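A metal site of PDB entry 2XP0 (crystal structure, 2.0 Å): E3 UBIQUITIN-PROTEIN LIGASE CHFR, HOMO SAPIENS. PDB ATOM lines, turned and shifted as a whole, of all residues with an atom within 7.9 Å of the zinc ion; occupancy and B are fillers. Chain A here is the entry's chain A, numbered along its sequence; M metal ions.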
ATOM      1  N   VAL A  36     -13.547 -24.284   3.475  1.00  0.00           N
ATOM      2  CA  VAL A  36     -14.065 -23.472   2.377  1.00  0.00           C
ATOM      3  C   VAL A  36     -15.362 -24.052   1.842  1.00  0.00           C
ATOM      4  O   VAL A  36     -15.435 -25.223   1.505  1.00  0.00           O
ATOM      5  CB  VAL A  36     -13.061 -23.371   1.211  1.00  0.00           C
ATOM      6  CG1 VAL A  36     -13.719 -22.753  -0.021  1.00  0.00           C
ATOM      7  CG2 VAL A  36     -11.840 -22.571   1.622  1.00  0.00           C
ATOM      8  N   VAL A  37     -16.388 -23.201   1.754  1.00  0.00           N
ATOM      9  CA  VAL A  37     -17.666 -23.608   1.185  1.00  0.00           C
ATOM     10  C   VAL A  37     -17.990 -22.708   0.001  1.00  0.00           C
ATOM     11  O   VAL A  37     -18.081 -21.487   0.162  1.00  0.00           O
ATOM     12  CB  VAL A  37     -18.791 -23.524   2.237  1.00  0.00           C
ATOM     13  CG1 VAL A  37     -20.099 -24.021   1.647  1.00  0.00           C
ATOM     14  CG2 VAL A  37     -18.417 -24.328   3.464  1.00  0.00           C
ATOM     15  N   CYS A  38     -18.162 -23.290  -1.189  1.00  0.00           N
ATOM     16  CA  CYS A  38     -18.488 -22.493  -2.378  1.00  0.00           C
ATOM     17  C   CYS A  38     -19.894 -22.787  -2.910  1.00  0.00           C
ATOM     18  O   CYS A  38     -20.601 -23.640  -2.387  1.00  0.00           O
ATOM     19  CB  CYS A  38     -17.447 -22.705  -3.492  1.00  0.00           C
ATOM     20  SG  CYS A  38     -17.680 -24.184  -4.531  1.00  0.00           S
ATOM     21  N   ARG A  39     -20.302 -22.061  -3.951  1.00  0.00           N
ATOM     22  CA  ARG A  39     -21.601 -22.273  -4.597  1.00  0.00           C
ATOM     23  C   ARG A  39     -21.932 -23.739  -4.882  1.00  0.00           C
ATOM     24  O   ARG A  39     -23.087 -24.138  -4.849  1.00  0.00           O
ATOM     25  CB  ARG A  39     -21.675 -21.496  -5.922  1.00  0.00           C
ATOM     26  CG  ARG A  39     -22.075 -20.035  -5.811  1.00  0.00           C
ATOM     27  CD  ARG A  39     -22.290 -19.432  -7.189  1.00  0.00           C
ATOM     28  NE  ARG A  39     -21.487 -18.231  -7.397  1.00  0.00           N
ATOM     29  CZ  ARG A  39     -21.424 -17.568  -8.553  1.00  0.00           C
ATOM     30  NH1 ARG A  39     -22.111 -18.011  -9.606  1.00  0.00           N
ATOM     31  NH2 ARG A  39     -20.678 -16.478  -8.667  1.00  0.00           N
ATOM     32  N   GLN A  40     -20.909 -24.532  -5.186  1.00  0.00           N
ATOM     33  CA  GLN A  40     -21.131 -25.906  -5.657  1.00  0.00           C
ATOM     34  C   GLN A  40     -20.743 -26.975  -4.636  1.00  0.00           C
ATOM     35  O   GLN A  40     -20.724 -28.167  -4.939  1.00  0.00           O
ATOM     36  CB  GLN A  40     -20.416 -26.128  -6.988  1.00  0.00           C
ATOM     37  CG  GLN A  40     -21.006 -25.283  -8.120  1.00  0.00           C
ATOM     38  CD  GLN A  40     -20.324 -25.519  -9.457  1.00  0.00           C
ATOM     39  OE1 GLN A  40     -19.159 -25.908  -9.508  1.00  0.00           O
ATOM     40  NE2 GLN A  40     -21.050 -25.283 -10.541  1.00  0.00           N
ATOM     41  N   CYS A  41     -20.431 -26.517  -3.430  1.00  0.00           N
ATOM     42  CA  CYS A  41     -20.156 -27.424  -2.319  1.00  0.00           C
ATOM     43  C   CYS A  41     -21.434 -28.127  -1.874  1.00  0.00           C
ATOM     44  O   CYS A  41     -22.508 -27.515  -1.856  1.00  0.00           O
ATOM     45  CB  CYS A  41     -19.537 -26.653  -1.149  1.00  0.00           C
ATOM     46  SG  CYS A  41     -17.733 -26.544  -1.163  1.00  0.00           S
ATOM     47  N   PRO A  42     -21.322 -29.425  -1.522  1.00  0.00           N
ATOM     48  CA  PRO A  42     -22.462 -30.211  -1.030  1.00  0.00           C
ATOM     49  C   PRO A  42     -23.004 -29.661   0.288  1.00  0.00           C
ATOM     50  O   PRO A  42     -22.247 -29.056   1.052  1.00  0.00           O
ATOM     51  CB  PRO A  42     -21.848 -31.605  -0.805  1.00  0.00           C
ATOM     52  CG  PRO A  42     -20.403 -31.343  -0.590  1.00  0.00           C
ATOM     53  CD  PRO A  42     -20.071 -30.194  -1.499  1.00  0.00           C
ATOM     54  N   ARG A  45     -21.214 -30.159   3.797  1.00  0.00           N
ATOM     55  CA  ARG A  45     -20.096 -29.266   4.008  1.00  0.00           C
ATOM     56  C   ARG A  45     -20.570 -27.958   4.641  1.00  0.00           C
ATOM     57  O   ARG A  45     -19.996 -27.484   5.613  1.00  0.00           O
ATOM     58  CB  ARG A  45     -19.389 -28.941   2.683  1.00  0.00           C
ATOM     59  CG  ARG A  45     -18.504 -30.061   2.153  1.00  0.00           C
ATOM     60  CD  ARG A  45     -17.082 -29.941   2.674  1.00  0.00           C
ATOM     61  NE  ARG A  45     -16.329 -28.866   2.035  1.00  0.00           N
ATOM     62  CZ  ARG A  45     -15.081 -28.552   2.343  1.00  0.00           C
ATOM     63  NH1 ARG A  45     -14.433 -29.219   3.295  1.00  0.00           N
ATOM     64  NH2 ARG A  45     -14.458 -27.566   1.704  1.00  0.00           N
ATOM     65  N   TYR A  84     -22.349 -29.426 -11.242  1.00  0.00           N
ATOM     66  CA  TYR A  84     -21.152 -29.938 -10.579  1.00  0.00           C
ATOM     67  C   TYR A  84     -21.222 -29.833  -9.053  1.00  0.00           C
ATOM     68  O   TYR A  84     -21.731 -28.839  -8.518  1.00  0.00           O
ATOM     69  CB  TYR A  84     -19.914 -29.198 -11.111  1.00  0.00           C
ATOM     70  CG  TYR A  84     -18.595 -29.707 -10.572  1.00  0.00           C
ATOM     71  CD1 TYR A  84     -17.978 -29.085  -9.505  1.00  0.00           C
ATOM     72  CD2 TYR A  84     -17.948 -30.788 -11.169  1.00  0.00           C
ATOM     73  CE1 TYR A  84     -16.762 -29.534  -9.019  1.00  0.00           C
ATOM     74  CE2 TYR A  84     -16.725 -31.245 -10.692  1.00  0.00           C
ATOM     75  CZ  TYR A  84     -16.141 -30.606  -9.623  1.00  0.00           C
ATOM     76  OH  TYR A  84     -14.927 -31.034  -9.134  1.00  0.00           O
ATOM     77  N   VAL A  85     -20.707 -30.855  -8.376  1.00  0.00           N
ATOM     78  CA  VAL A  85     -20.638 -30.859  -6.915  1.00  0.00           C
ATOM     79  C   VAL A  85     -19.228 -31.212  -6.456  1.00  0.00           C
ATOM     80  O   VAL A  85     -18.660 -32.201  -6.898  1.00  0.00           O
ATOM     81  CB  VAL A  85     -21.625 -31.866  -6.298  1.00  0.00           C
ATOM     82  CG1 VAL A  85     -21.467 -31.881  -4.782  1.00  0.00           C
ATOM     83  CG2 VAL A  85     -23.050 -31.519  -6.689  1.00  0.00           C
ATOM     84  N   CYS A  86     -18.684 -30.385  -5.564  1.00  0.00           N
ATOM     85  CA  CYS A  86     -17.311 -30.548  -5.112  1.00  0.00           C
ATOM     86  C   CYS A  86     -17.043 -31.870  -4.380  1.00  0.00           C
ATOM     87  O   CYS A  86     -17.669 -32.157  -3.357  1.00  0.00           O
ATOM     88  CB  CYS A  86     -16.907 -29.368  -4.222  1.00  0.00           C
ATOM     89  SG  CYS A  86     -17.088 -27.754  -5.002  1.00  0.00           S
ATOM     90  N   PRO A  87     -16.097 -32.656  -4.904  1.00  0.00           N
ATOM     91  CA  PRO A  87     -15.612 -33.917  -4.314  1.00  0.00           C
ATOM     92  C   PRO A  87     -14.709 -33.662  -3.104  1.00  0.00           C
ATOM     93  O   PRO A  87     -14.192 -32.556  -2.950  1.00  0.00           O
ATOM     94  CB  PRO A  87     -14.791 -34.530  -5.444  1.00  0.00           C
ATOM     95  CG  PRO A  87     -14.307 -33.359  -6.213  1.00  0.00           C
ATOM     96  CD  PRO A  87     -15.459 -32.398  -6.203  1.00  0.00           C
ATOM     97  N   GLY A  90     -11.109 -32.792  -4.090  1.00  0.00           N
ATOM     98  CA  GLY A  90     -10.996 -31.624  -4.944  1.00  0.00           C
ATOM     99  C   GLY A  90     -10.549 -30.401  -4.149  1.00  0.00           C
ATOM    100  O   GLY A  90     -10.527 -30.431  -2.920  1.00  0.00           O
ATOM    101  N   SER A  91     -10.211 -29.325  -4.850  1.00  0.00           N
ATOM    102  CA  SER A  91      -9.755 -28.109  -4.196  1.00  0.00           C
ATOM    103  C   SER A  91     -10.485 -26.877  -4.726  1.00  0.00           C
ATOM    104  O   SER A  91     -11.273 -26.976  -5.660  1.00  0.00           O
ATOM    105  CB  SER A  91      -8.242 -27.955  -4.352  1.00  0.00           C
ATOM    106  OG  SER A  91      -7.871 -27.963  -5.720  1.00  0.00           O
ATOM    107  N   HIS A  92     -10.231 -25.719  -4.106  1.00  0.00           N
ATOM    108  CA  HIS A  92     -10.850 -24.468  -4.520  1.00  0.00           C
ATOM    109  C   HIS A  92      -9.803 -23.435  -4.873  1.00  0.00           C
ATOM    110  O   HIS A  92      -8.684 -23.450  -4.337  1.00  0.00           O
ATOM    111  CB  HIS A  92     -11.744 -23.922  -3.401  1.00  0.00           C
ATOM    112  CG  HIS A  92     -12.930 -24.785  -3.099  1.00  0.00           C
ATOM    113  ND1 HIS A  92     -12.893 -25.785  -2.147  1.00  0.00           N
ATOM    114  CD2 HIS A  92     -14.184 -24.805  -3.606  1.00  0.00           C
ATOM    115  CE1 HIS A  92     -14.066 -26.379  -2.084  1.00  0.00           C
ATOM    116  NE2 HIS A  92     -14.878 -25.810  -2.959  1.00  0.00           N
ATOM    117  N   PRO A 101     -14.562 -18.215  -3.624  1.00  0.00           N
ATOM    118  CA  PRO A 101     -14.046 -19.538  -3.998  1.00  0.00           C
ATOM    119  C   PRO A 101     -14.876 -20.197  -5.093  1.00  0.00           C
ATOM    120  O   PRO A 101     -16.089 -20.058  -5.127  1.00  0.00           O
ATOM    121  CB  PRO A 101     -14.202 -20.342  -2.711  1.00  0.00           C
ATOM    122  CG  PRO A 101     -15.328 -19.675  -1.999  1.00  0.00           C
ATOM    123  CD  PRO A 101     -15.103 -18.224  -2.251  1.00  0.00           C
ATOM    124  N   MET A 102     -14.187 -20.896  -5.982  1.00  0.00           N
ATOM    125  CA  MET A 102     -14.835 -21.764  -6.956  1.00  0.00           C
ATOM    126  C   MET A 102     -14.014 -23.049  -6.966  1.00  0.00           C
ATOM    127  O   MET A 102     -12.853 -23.056  -6.565  1.00  0.00           O
ATOM    128  CB  MET A 102     -14.806 -21.122  -8.335  1.00  0.00           C
ATOM    129  CG  MET A 102     -13.402 -20.900  -8.876  1.00  0.00           C
ATOM    130  SD  MET A 102     -13.331 -20.038 -10.462  1.00  0.00           S
ATOM    131  CE  MET A 102     -11.567 -19.803 -10.592  1.00  0.00           C
ATOM    132  N   PRO A 103     -14.623 -24.154  -7.403  1.00  0.00           N
ATOM    133  CA  PRO A 103     -13.839 -25.389  -7.465  1.00  0.00           C
ATOM    134  C   PRO A 103     -12.701 -25.221  -8.467  1.00  0.00           C
ATOM    135  O   PRO A 103     -12.929 -24.656  -9.537  1.00  0.00           O
ATOM    136  CB  PRO A 103     -14.843 -26.417  -7.997  1.00  0.00           C
ATOM    137  CG  PRO A 103     -15.918 -25.619  -8.650  1.00  0.00           C
ATOM    138  CD  PRO A 103     -15.993 -24.321  -7.917  1.00  0.00           C
ATOM    139  N   ASP A 104     -11.498 -25.666  -8.116  1.00  0.00           N
ATOM    140  CA  ASP A 104     -10.370 -25.535  -9.019  1.00  0.00           C
ATOM    141  C   ASP A 104     -10.299 -26.717  -9.972  1.00  0.00           C
ATOM    142  O   ASP A 104      -9.798 -27.779  -9.606  1.00  0.00           O
ATOM    143  CB  ASP A 104      -9.056 -25.401  -8.252  1.00  0.00           C
ATOM    144  CG  ASP A 104      -7.891 -25.067  -9.164  1.00  0.00           C
ATOM    145  OD1 ASP A 104      -6.841 -24.637  -8.639  1.00  0.00           O
ATOM    146  OD2 ASP A 104      -8.024 -25.211 -10.395  1.00  0.00           O
ATOM    147  N   TRP A 132     -19.073 -19.696 -13.944  1.00  0.00           N
ATOM    148  CA  TRP A 132     -20.427 -19.629 -13.382  1.00  0.00           C
ATOM    149  C   TRP A 132     -21.027 -18.237 -13.194  1.00  0.00           C
ATOM    150  O   TRP A 132     -22.073 -18.094 -12.572  1.00  0.00           O
ATOM    151  CB  TRP A 132     -20.516 -20.438 -12.065  1.00  0.00           C
ATOM    152  CG  TRP A 132     -19.678 -19.912 -10.910  1.00  0.00           C
ATOM    153  CD1 TRP A 132     -19.124 -18.673 -10.786  1.00  0.00           C
ATOM    154  CD2 TRP A 132     -19.328 -20.631  -9.718  1.00  0.00           C
ATOM    155  NE1 TRP A 132     -18.438 -18.578  -9.596  1.00  0.00           N
ATOM    156  CE2 TRP A 132     -18.547 -19.762  -8.925  1.00  0.00           C
ATOM    157  CE3 TRP A 132     -19.570 -21.931  -9.248  1.00  0.00           C
ATOM    158  CZ2 TRP A 132     -18.025 -20.149  -7.691  1.00  0.00           C
ATOM    159  CZ3 TRP A 132     -19.054 -22.308  -8.028  1.00  0.00           C
ATOM    160  CH2 TRP A 132     -18.285 -21.423  -7.259  1.00  0.00           C
HETATM  161 ZN    ZN M   1     -16.933 -26.055  -3.391  1.00  0.00          ZN
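The side-chain sulfur (SG) of Cys 38 sits close to the backbone NH (N) of Gln 40 (3.3 Å).
O of Gln 40 sits at hydrogen-bond distance from N of Cys 86 (3.1 Å).
The backbone carbonyl oxygen of Val 36 lies close to the side-chain sulfur of Cys 41 (3.8 Å).
Within 4 Å of the zinc ion: Cys 38, Cys 41, Cys 86 and His 92.
The nearest printed residue that does not touch the zinc ion is Gln 40 (4.1 Å).
The zinc ion is bound by a ring nitrogen (NE2) of His 92 (2.1 Å), the side-chain sulfur (SG) of Cys 38 (2.3 Å), the side-chain sulfur (SG) of Cys 86 (2.3 Å) and the side-chain sulfur (SG) of Cys 41 (2.4 Å).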
